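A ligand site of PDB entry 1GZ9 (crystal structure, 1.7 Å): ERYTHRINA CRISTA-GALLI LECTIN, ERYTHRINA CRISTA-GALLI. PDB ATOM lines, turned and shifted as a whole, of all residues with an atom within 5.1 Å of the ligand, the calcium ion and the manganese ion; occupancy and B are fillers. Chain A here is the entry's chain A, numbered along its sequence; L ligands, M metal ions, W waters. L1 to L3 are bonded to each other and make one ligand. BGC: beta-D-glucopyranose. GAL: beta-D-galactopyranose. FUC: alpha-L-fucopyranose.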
ATOM      1  N   LEU A  86     -31.889 -13.329   0.113  1.00  0.00           N
ATOM      2  CA  LEU A  86     -32.417 -14.665   0.484  1.00  0.00           C
ATOM      3  C   LEU A  86     -31.276 -15.465   1.121  1.00  0.00           C
ATOM      4  O   LEU A  86     -30.126 -15.369   0.696  1.00  0.00           O
ATOM      5  CB  LEU A  86     -32.880 -15.411  -0.760  1.00  0.00           C
ATOM      6  CG  LEU A  86     -34.145 -14.854  -1.430  1.00  0.00           C
ATOM      7  CD1 LEU A  86     -34.430 -15.689  -2.701  1.00  0.00           C
ATOM      8  CD2 LEU A  86     -35.331 -14.879  -0.471  1.00  0.00           C
ATOM      9  N   ALA A  88     -28.884 -18.798   2.120  1.00  0.00           N
ATOM     10  CA  ALA A  88     -28.357 -19.908   1.287  1.00  0.00           C
ATOM     11  C   ALA A  88     -27.189 -20.503   2.065  1.00  0.00           C
ATOM     12  O   ALA A  88     -26.689 -19.843   2.980  1.00  0.00           O
ATOM     13  CB  ALA A  88     -27.869 -19.367  -0.049  1.00  0.00           C
ATOM     14  N   ASP A  89     -26.751 -21.731   1.778  1.00  0.00           N
ATOM     15  CA  ASP A  89     -27.302 -22.628   0.753  1.00  0.00           C
ATOM     16  C   ASP A  89     -27.851 -23.956   1.353  1.00  0.00           C
ATOM     17  O   ASP A  89     -28.729 -24.584   0.748  1.00  0.00           O
ATOM     18  CB  ASP A  89     -26.219 -22.965  -0.265  1.00  0.00           C
ATOM     19  CG  ASP A  89     -26.258 -22.065  -1.508  1.00  0.00           C
ATOM     20  OD1 ASP A  89     -27.180 -22.222  -2.349  1.00  0.00           O
ATOM     21  OD2 ASP A  89     -25.356 -21.192  -1.643  1.00  0.00           O
ATOM     22  N   TYR A 106     -21.616 -23.170  -2.603  1.00  0.00           N
ATOM     23  CA  TYR A 106     -22.912 -22.591  -2.905  1.00  0.00           C
ATOM     24  C   TYR A 106     -23.957 -23.692  -2.991  1.00  0.00           C
ATOM     25  O   TYR A 106     -23.949 -24.599  -2.148  1.00  0.00           O
ATOM     26  CB  TYR A 106     -22.845 -21.804  -4.216  1.00  0.00           C
ATOM     27  CG  TYR A 106     -21.650 -20.889  -4.211  1.00  0.00           C
ATOM     28  CD1 TYR A 106     -21.396 -20.058  -3.115  1.00  0.00           C
ATOM     29  CD2 TYR A 106     -20.823 -20.797  -5.324  1.00  0.00           C
ATOM     30  CE1 TYR A 106     -20.349 -19.137  -3.134  1.00  0.00           C
ATOM     31  CE2 TYR A 106     -19.757 -19.868  -5.357  1.00  0.00           C
ATOM     32  CZ  TYR A 106     -19.539 -19.048  -4.265  1.00  0.00           C
ATOM     33  OH  TYR A 106     -18.501 -18.118  -4.308  1.00  0.00           O
ATOM     34  N   GLY A 107     -24.803 -23.638  -4.016  1.00  0.00           N
ATOM     35  CA  GLY A 107     -25.873 -24.614  -4.152  1.00  0.00           C
ATOM     36  C   GLY A 107     -25.400 -26.056  -4.384  1.00  0.00           C
ATOM     37  O   GLY A 107     -26.220 -26.999  -4.333  1.00  0.00           O
ATOM     38  N   TYR A 108     -24.113 -26.257  -4.617  1.00  0.00           N
ATOM     39  CA  TYR A 108     -23.599 -27.608  -4.834  1.00  0.00           C
ATOM     40  C   TYR A 108     -23.218 -28.273  -3.518  1.00  0.00           C
ATOM     41  O   TYR A 108     -22.816 -29.454  -3.491  1.00  0.00           O
ATOM     42  CB  TYR A 108     -22.413 -27.583  -5.793  1.00  0.00           C
ATOM     43  CG  TYR A 108     -22.792 -26.900  -7.096  1.00  0.00           C
ATOM     44  CD1 TYR A 108     -23.578 -27.542  -8.045  1.00  0.00           C
ATOM     45  CD2 TYR A 108     -22.418 -25.558  -7.342  1.00  0.00           C
ATOM     46  CE1 TYR A 108     -23.993 -26.890  -9.214  1.00  0.00           C
ATOM     47  CE2 TYR A 108     -22.830 -24.896  -8.509  1.00  0.00           C
ATOM     48  CZ  TYR A 108     -23.617 -25.576  -9.430  1.00  0.00           C
ATOM     49  OH  TYR A 108     -24.077 -24.910 -10.551  1.00  0.00           O
ATOM     50  N   GLU A 127     -29.900 -33.959   1.614  1.00  0.00           N
ATOM     51  CA  GLU A 127     -29.732 -32.511   1.785  1.00  0.00           C
ATOM     52  C   GLU A 127     -30.862 -31.833   2.530  1.00  0.00           C
ATOM     53  O   GLU A 127     -31.970 -32.356   2.569  1.00  0.00           O
ATOM     54  CB  GLU A 127     -29.598 -31.878   0.407  1.00  0.00           C
ATOM     55  CG  GLU A 127     -30.860 -32.012  -0.467  1.00  0.00           C
ATOM     56  CD  GLU A 127     -30.820 -31.172  -1.740  1.00  0.00           C
ATOM     57  OE1 GLU A 127     -29.806 -31.215  -2.504  1.00  0.00           O
ATOM     58  OE2 GLU A 127     -31.845 -30.502  -1.948  1.00  0.00           O
ATOM     59  N   ASP A 129     -31.841 -28.261   2.119  1.00  0.00           N
ATOM     60  CA  ASP A 129     -31.527 -27.160   1.176  1.00  0.00           C
ATOM     61  C   ASP A 129     -32.347 -25.930   1.433  1.00  0.00           C
ATOM     62  O   ASP A 129     -33.579 -26.001   1.474  1.00  0.00           O
ATOM     63  CB  ASP A 129     -31.803 -27.742  -0.236  1.00  0.00           C
ATOM     64  CG  ASP A 129     -31.358 -26.838  -1.377  1.00  0.00           C
ATOM     65  OD1 ASP A 129     -31.022 -25.681  -1.130  1.00  0.00           O
ATOM     66  OD2 ASP A 129     -31.377 -27.331  -2.529  1.00  0.00           O
ATOM     67  N   PHE A 131     -31.944 -22.783  -0.373  1.00  0.00           N
ATOM     68  CA  PHE A 131     -32.032 -21.786  -1.464  1.00  0.00           C
ATOM     69  C   PHE A 131     -32.474 -22.483  -2.716  1.00  0.00           C
ATOM     70  O   PHE A 131     -31.856 -23.484  -3.113  1.00  0.00           O
ATOM     71  CB  PHE A 131     -30.656 -21.149  -1.699  1.00  0.00           C
ATOM     72  CG  PHE A 131     -30.660 -20.122  -2.839  1.00  0.00           C
ATOM     73  CD1 PHE A 131     -30.922 -18.789  -2.590  1.00  0.00           C
ATOM     74  CD2 PHE A 131     -30.427 -20.546  -4.154  1.00  0.00           C
ATOM     75  CE1 PHE A 131     -30.963 -17.854  -3.658  1.00  0.00           C
ATOM     76  CE2 PHE A 131     -30.471 -19.620  -5.224  1.00  0.00           C
ATOM     77  CZ  PHE A 131     -30.742 -18.283  -4.978  1.00  0.00           C
ATOM     78  N   SER A 132     -33.479 -21.927  -3.392  1.00  0.00           N
ATOM     79  CA  SER A 132     -34.017 -22.582  -4.612  1.00  0.00           C
ATOM     80  C   SER A 132     -33.188 -22.216  -5.857  1.00  0.00           C
ATOM     81  O   SER A 132     -33.339 -21.114  -6.431  1.00  0.00           O
ATOM     82  CB  SER A 132     -35.472 -22.161  -4.853  1.00  0.00           C
ATOM     83  OG  SER A 132     -36.054 -22.940  -5.888  1.00  0.00           O
ATOM     84  N   ASN A 133     -32.310 -23.128  -6.229  1.00  0.00           N
ATOM     85  CA  ASN A 133     -31.459 -22.970  -7.434  1.00  0.00           C
ATOM     86  C   ASN A 133     -32.292 -23.336  -8.694  1.00  0.00           C
ATOM     87  O   ASN A 133     -33.398 -23.854  -8.589  1.00  0.00           O
ATOM     88  CB  ASN A 133     -30.270 -23.931  -7.334  1.00  0.00           C
ATOM     89  CG  ASN A 133     -29.300 -23.512  -6.252  1.00  0.00           C
ATOM     90  OD1 ASN A 133     -29.410 -23.922  -5.088  1.00  0.00           O
ATOM     91  ND2 ASN A 133     -28.350 -22.633  -6.616  1.00  0.00           N
ATOM     92  N   PRO A 134     -31.739 -23.124  -9.890  1.00  0.00           N
ATOM     93  CA  PRO A 134     -32.470 -23.440 -11.127  1.00  0.00           C
ATOM     94  C   PRO A 134     -32.924 -24.906 -11.271  1.00  0.00           C
ATOM     95  O   PRO A 134     -33.857 -25.190 -12.054  1.00  0.00           O
ATOM     96  CB  PRO A 134     -31.463 -23.041 -12.233  1.00  0.00           C
ATOM     97  CG  PRO A 134     -30.706 -21.885 -11.585  1.00  0.00           C
ATOM     98  CD  PRO A 134     -30.475 -22.411 -10.171  1.00  0.00           C
ATOM     99  N   TRP A 135     -32.305 -25.832 -10.527  1.00  0.00           N
ATOM    100  CA  TRP A 135     -32.632 -27.246 -10.593  1.00  0.00           C
ATOM    101  C   TRP A 135     -33.487 -27.699  -9.401  1.00  0.00           C
ATOM    102  O   TRP A 135     -33.817 -28.905  -9.296  1.00  0.00           O
ATOM    103  CB  TRP A 135     -31.342 -28.094 -10.561  1.00  0.00           C
ATOM    104  CG  TRP A 135     -30.482 -27.777  -9.306  1.00  0.00           C
ATOM    105  CD1 TRP A 135     -30.672 -28.256  -8.020  1.00  0.00           C
ATOM    106  CD2 TRP A 135     -29.354 -26.898  -9.245  1.00  0.00           C
ATOM    107  NE1 TRP A 135     -29.726 -27.716  -7.160  1.00  0.00           N
ATOM    108  CE2 TRP A 135     -28.902 -26.888  -7.891  1.00  0.00           C
ATOM    109  CE3 TRP A 135     -28.673 -26.116 -10.199  1.00  0.00           C
ATOM    110  CZ2 TRP A 135     -27.801 -26.120  -7.486  1.00  0.00           C
ATOM    111  CZ3 TRP A 135     -27.588 -25.356  -9.789  1.00  0.00           C
ATOM    112  CH2 TRP A 135     -27.151 -25.376  -8.424  1.00  0.00           C
ATOM    113  N   ASP A 136     -33.812 -26.756  -8.519  1.00  0.00           N
ATOM    114  CA  ASP A 136     -34.580 -27.070  -7.299  1.00  0.00           C
ATOM    115  C   ASP A 136     -36.071 -26.850  -7.360  1.00  0.00           C
ATOM    116  O   ASP A 136     -36.561 -26.113  -8.193  1.00  0.00           O
ATOM    117  CB  ASP A 136     -34.145 -26.139  -6.131  1.00  0.00           C
ATOM    118  CG  ASP A 136     -32.864 -26.600  -5.434  1.00  0.00           C
ATOM    119  OD1 ASP A 136     -32.740 -27.794  -5.172  1.00  0.00           O
ATOM    120  OD2 ASP A 136     -32.005 -25.745  -5.146  1.00  0.00           O
ATOM    121  N   PRO A 137     -36.822 -27.486  -6.438  1.00  0.00           N
ATOM    122  CA  PRO A 137     -38.260 -27.287  -6.384  1.00  0.00           C
ATOM    123  C   PRO A 137     -38.316 -25.889  -5.788  1.00  0.00           C
ATOM    124  O   PRO A 137     -37.336 -25.417  -5.193  1.00  0.00           O
ATOM    125  CB  PRO A 137     -38.733 -28.333  -5.378  1.00  0.00           C
ATOM    126  CG  PRO A 137     -37.507 -28.596  -4.540  1.00  0.00           C
ATOM    127  CD  PRO A 137     -36.423 -28.628  -5.588  1.00  0.00           C
ATOM    128  N   HIS A 142     -36.069 -27.470   1.884  1.00  0.00           N
ATOM    129  CA  HIS A 142     -36.599 -28.783   1.544  1.00  0.00           C
ATOM    130  C   HIS A 142     -35.559 -29.869   1.874  1.00  0.00           C
ATOM    131  O   HIS A 142     -34.350 -29.628   1.919  1.00  0.00           O
ATOM    132  CB  HIS A 142     -37.038 -28.892   0.045  1.00  0.00           C
ATOM    133  CG  HIS A 142     -35.965 -28.570  -0.947  1.00  0.00           C
ATOM    134  ND1 HIS A 142     -35.874 -27.330  -1.552  1.00  0.00           N
ATOM    135  CD2 HIS A 142     -34.962 -29.307  -1.457  1.00  0.00           C
ATOM    136  CE1 HIS A 142     -34.850 -27.318  -2.382  1.00  0.00           C
ATOM    137  NE2 HIS A 142     -34.272 -28.509  -2.352  1.00  0.00           N
ATOM    138  N   ILE A 150     -26.948 -33.186  -7.788  1.00  0.00           N
ATOM    139  CA  ILE A 150     -27.500 -32.184  -6.868  1.00  0.00           C
ATOM    140  C   ILE A 150     -29.019 -32.014  -7.194  1.00  0.00           C
ATOM    141  O   ILE A 150     -29.781 -31.407  -6.421  1.00  0.00           O
ATOM    142  CB  ILE A 150     -26.786 -30.807  -7.054  1.00  0.00           C
ATOM    143  CG1 ILE A 150     -27.191 -29.843  -5.919  1.00  0.00           C
ATOM    144  CG2 ILE A 150     -27.147 -30.197  -8.390  1.00  0.00           C
ATOM    145  CD1 ILE A 150     -26.741 -30.320  -4.534  1.00  0.00           C
ATOM    146  N   SER A 152     -32.241 -33.448  -6.968  1.00  0.00           N
ATOM    147  CA  SER A 152     -32.831 -34.546  -6.196  1.00  0.00           C
ATOM    148  C   SER A 152     -33.819 -35.434  -6.927  1.00  0.00           C
ATOM    149  O   SER A 152     -34.639 -34.922  -7.697  1.00  0.00           O
ATOM    150  CB  SER A 152     -33.570 -33.981  -4.987  1.00  0.00           C
ATOM    151  OG  SER A 152     -32.705 -33.173  -4.216  1.00  0.00           O
ATOM    152  N   THR A 155     -37.970 -34.718  -3.180  1.00  0.00           N
ATOM    153  CA  THR A 155     -37.816 -33.682  -2.154  1.00  0.00           C
ATOM    154  C   THR A 155     -39.064 -33.580  -1.302  1.00  0.00           C
ATOM    155  O   THR A 155     -40.149 -34.038  -1.679  1.00  0.00           O
ATOM    156  CB  THR A 155     -37.521 -32.266  -2.769  1.00  0.00           C
ATOM    157  OG1 THR A 155     -38.578 -31.910  -3.671  1.00  0.00           O
ATOM    158  CG2 THR A 155     -36.215 -32.281  -3.566  1.00  0.00           C
ATOM    159  N   THR A 216     -22.582 -21.591   2.502  1.00  0.00           N
ATOM    160  CA  THR A 216     -23.338 -20.336   2.474  1.00  0.00           C
ATOM    161  C   THR A 216     -23.198 -19.805   1.066  1.00  0.00           C
ATOM    162  O   THR A 216     -22.470 -20.391   0.250  1.00  0.00           O
ATOM    163  CB  THR A 216     -22.891 -19.290   3.540  1.00  0.00           C
ATOM    164  OG1 THR A 216     -21.487 -19.082   3.474  1.00  0.00           O
ATOM    165  CG2 THR A 216     -23.274 -19.807   4.920  1.00  0.00           C
ATOM    166  N   GLY A 217     -23.903 -18.711   0.781  1.00  0.00           N
ATOM    167  CA  GLY A 217     -24.025 -18.208  -0.581  1.00  0.00           C
ATOM    168  C   GLY A 217     -23.001 -17.403  -1.334  1.00  0.00           C
ATOM    169  O   GLY A 217     -21.993 -17.015  -0.780  1.00  0.00           O
ATOM    170  N   ALA A 218     -23.325 -17.148  -2.609  1.00  0.00           N
ATOM    171  CA  ALA A 218     -22.407 -16.469  -3.514  1.00  0.00           C
ATOM    172  C   ALA A 218     -22.471 -14.968  -3.558  1.00  0.00           C
ATOM    173  O   ALA A 218     -21.850 -14.359  -4.425  1.00  0.00           O
ATOM    174  CB  ALA A 218     -22.552 -17.044  -4.939  1.00  0.00           C
ATOM    175  N   GLN A 219     -23.220 -14.354  -2.650  1.00  0.00           N
ATOM    176  CA  GLN A 219     -23.240 -12.904  -2.617  1.00  0.00           C
ATOM    177  C   GLN A 219     -23.369 -12.499  -1.167  1.00  0.00           C
ATOM    178  O   GLN A 219     -23.787 -13.303  -0.317  1.00  0.00           O
ATOM    179  CB  GLN A 219     -24.389 -12.312  -3.453  1.00  0.00           C
ATOM    180  CG  GLN A 219     -25.770 -12.573  -2.898  1.00  0.00           C
ATOM    181  CD  GLN A 219     -26.861 -11.865  -3.710  1.00  0.00           C
ATOM    182  OE1 GLN A 219     -27.463 -10.898  -3.235  1.00  0.00           O
ATOM    183  NE2 GLN A 219     -27.119 -12.351  -4.911  1.00  0.00           N
ATOM    184  N   ALA A 222     -25.965 -13.709   1.885  1.00  0.00           N
ATOM    185  CA  ALA A 222     -26.853 -14.803   1.419  1.00  0.00           C
ATOM    186  C   ALA A 222     -26.229 -15.889   2.299  1.00  0.00           C
ATOM    187  O   ALA A 222     -25.383 -16.666   1.842  1.00  0.00           O
ATOM    188  CB  ALA A 222     -26.609 -15.102  -0.083  1.00  0.00           C
HETATM  189  C2  BGC L   1     -24.999 -13.573  -7.951  1.00  0.00           C
HETATM  190  C3  BGC L   1     -24.838 -14.898  -7.160  1.00  0.00           C
HETATM  191  C4  BGC L   1     -25.562 -16.044  -7.892  1.00  0.00           C
HETATM  192  C5  BGC L   1     -25.082 -16.179  -9.348  1.00  0.00           C
HETATM  193  C6  BGC L   1     -25.939 -17.152 -10.156  1.00  0.00           C
HETATM  194  C1  BGC L   1     -24.444 -13.803  -9.368  1.00  0.00           C
HETATM  195  O1  BGC L   1     -24.592 -12.624 -10.095  1.00  0.00           O
HETATM  196  O2  BGC L   1     -24.273 -12.555  -7.265  1.00  0.00           O
HETATM  197  O3  BGC L   1     -25.345 -14.710  -5.859  1.00  0.00           O
HETATM  198  O4  BGC L   1     -25.259 -17.367  -7.250  1.00  0.00           O
HETATM  199  O5  BGC L   1     -25.217 -14.879 -10.014  1.00  0.00           O
HETATM  200  O6  BGC L   1     -25.186 -17.655 -11.277  1.00  0.00           O
HETATM  201  C1  GAL L   2     -26.262 -17.954  -6.357  1.00  0.00           C
HETATM  202  C2  GAL L   2     -25.816 -19.351  -6.141  1.00  0.00           C
HETATM  203  C3  GAL L   2     -26.914 -19.958  -5.126  1.00  0.00           C
HETATM  204  C4  GAL L   2     -26.912 -19.131  -3.826  1.00  0.00           C
HETATM  205  C5  GAL L   2     -27.272 -17.676  -4.227  1.00  0.00           C
HETATM  206  C6  GAL L   2     -27.280 -16.739  -3.070  1.00  0.00           C
HETATM  207  O2  GAL L   2     -25.902 -19.974  -7.430  1.00  0.00           O
HETATM  208  O3  GAL L   2     -26.541 -21.338  -4.841  1.00  0.00           O
HETATM  209  O4  GAL L   2     -25.630 -19.109  -3.194  1.00  0.00           O
HETATM  210  O5  GAL L   2     -26.289 -17.180  -5.160  1.00  0.00           O
HETATM  211  O6  GAL L   2     -27.754 -15.481  -3.581  1.00  0.00           O
HETATM  212  C1  FUC L   3     -25.368 -21.244  -7.750  1.00  0.00           C
HETATM  213  C2  FUC L   3     -26.009 -21.590  -9.117  1.00  0.00           C
HETATM  214  C3  FUC L   3     -25.483 -20.813 -10.369  1.00  0.00           C
HETATM  215  C4  FUC L   3     -23.921 -20.694 -10.340  1.00  0.00           C
HETATM  216  C5  FUC L   3     -23.458 -20.127  -8.965  1.00  0.00           C
HETATM  217  C6  FUC L   3     -21.883 -19.997  -8.865  1.00  0.00           C
HETATM  218  O2  FUC L   3     -27.431 -21.826  -8.996  1.00  0.00           O
HETATM  219  O3  FUC L   3     -25.885 -21.531 -11.533  1.00  0.00           O
HETATM  220  O4  FUC L   3     -23.343 -21.973 -10.536  1.00  0.00           O
HETATM  221  O5  FUC L   3     -23.906 -21.032  -7.815  1.00  0.00           O
HETATM  222 CA    CA M   1     -30.386 -25.327  -3.444  1.00  0.00          CA
HETATM  223 MN    MN M   2     -32.336 -29.026  -3.499  1.00  0.00          MN
HETATM  224  O   HOH W   1     -29.482 -14.503  -1.958  1.00  0.00           O
HETATM  225  O   HOH W   2     -20.833 -22.220 -11.267  1.00  0.00           O
HETATM  226  O   HOH W   3     -22.347 -17.268 -11.660  1.00  0.00           O
HETATM  227  O   HOH W   4     -21.625 -11.990  -5.814  1.00  0.00           O
HETATM  228  O   HOH W   5     -28.985 -27.147  -4.165  1.00  0.00           O
HETATM  229  O   HOH W   6     -27.790 -15.294 -12.422  1.00  0.00           O
HETATM  230  O   HOH W   7     -28.679 -19.360  -9.115  1.00  0.00           O
HETATM  231  O   HOH W   8     -33.342 -30.582  -4.698  1.00  0.00           O
HETATM  232  O   HOH W   9     -30.263 -29.570  -4.422  1.00  0.00           O
HETATM  233  O   HOH W  10     -28.773 -24.282  -2.053  1.00  0.00           O
HETATM  234  O   HOH W  11     -29.108 -15.177  -6.137  1.00  0.00           O
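The side-chain carboxylate (OD2) of Asp 89 sits at hydrogen-bond distance from an oxygen (O4) of GAL L2 (2.6 Å).
The backbone NH (N) of Gly 107 lies within hydrogen-bond range of an oxygen (O3) of GAL L2, 3.0 Å away.
An oxygen (O4) of GAL L2 sits at hydrogen-bond distance from the backbone NH (N) of Ala 218, at 3.1 Å.
An oxygen (O2) of FUC L3 is in hydrogen-bond range of the side-chain amide nitrogen (ND2) of Asn 133 (2.7 Å).
NE2 of Gln 219 sits at hydrogen-bond distance from O3 of BGC L1 (3.1 Å).
The side-chain hydroxyl of Tyr 108 lies within hydrogen-bond range of an oxygen (O4) of FUC L3 (3.0 Å).
The side-chain carboxylate (OD1) of Asp 89 lies within hydrogen-bond range of the backbone NH (N) of Gly 107, 3.2 Å away.
The backbone carbonyl oxygen (O) of Ala 222 sits at hydrogen-bond distance from the backbone NH (N) of Gly 217 (2.7 Å).
Ala 88 touches the ligand.
Tyr 106 touches the ligand.
CD of Pro 134 touches O2 of FUC L3 (3.3 Å).
CH2 of Trp 135 touches O2 of FUC L3, 3.6 Å away.
Gly 217 touches the ligand.
CB of Ala 222 touches C6 of GAL L2 (3.5 Å).
Hydrophobic or aromatic side chains that line the ligand: Ala 88, Tyr 106, Tyr 108, Phe 131, Pro 134, Trp 135, Ala 218 and Ala 222.
Within 4 Å of the ligand: Ala 88, Asp 89, Tyr 106, Gly 107, Tyr 108, Phe 131, Asn 133, Pro 134, Trp 135, Gly 217, Ala 218, Gln 219 and Ala 222.
The nearest printed residue that does not touch the ligand is Thr 216 (4.8 Å).
Within 4 Å of the calcium ion: Asp 129, Phe 131, Asn 133 and Asp 136.
Within 4 Å of the manganese ion: Glu 127, Asp 129, Asp 136 and His 142.
The nearest printed residue that does not touch the manganese ion is Ser 152 (4.2 Å).
Water W10 binds the calcium ion (2.4 Å).
OD1 of Asn 133 binds the calcium ion.
O of Phe 131 is bound to the calcium ion (2.4 Å).
OD2 of Asp 136 is bound to the calcium ion (2.4 Å).
The calcium ion is bound by water W5, 2.4 Å away.
The side-chain carboxylate (OD2) of Asp 129 binds the calcium ion (2.4 Å).
The calcium ion is bound by OD1 of Asp 129 (2.4 Å).
The calcium ion has seven donor atoms within binding distance.
The manganese ion is bound by OD1 of Asp 136 (2.1 Å), OD2 of Asp 129 (2.2 Å), OE2 of Glu 127 (2.2 Å), water W8 (2.2 Å), NE2 of His 142 (2.3 Å) and water W9 (2.3 Å).
Water W5 bridges O of Gly 107 and NE1 of Trp 135.
Water W9 lies within hydrogen-bond range of the side-chain carboxylate (OE1) of Glu 127, the backbone carbonyl oxygen (O) of Ile 150 and the indole nitrogen (NE1) of Trp 135.
Water W1 lies within hydrogen-bond range of an oxygen (O6) of GAL L2 (2.6 Å) and the backbone carbonyl oxygen of Leu 86 (2.9 Å).
Water W4 bridges O of Ala 218 (2.8 Å) and O2 of BGC L1 (3.1 Å).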
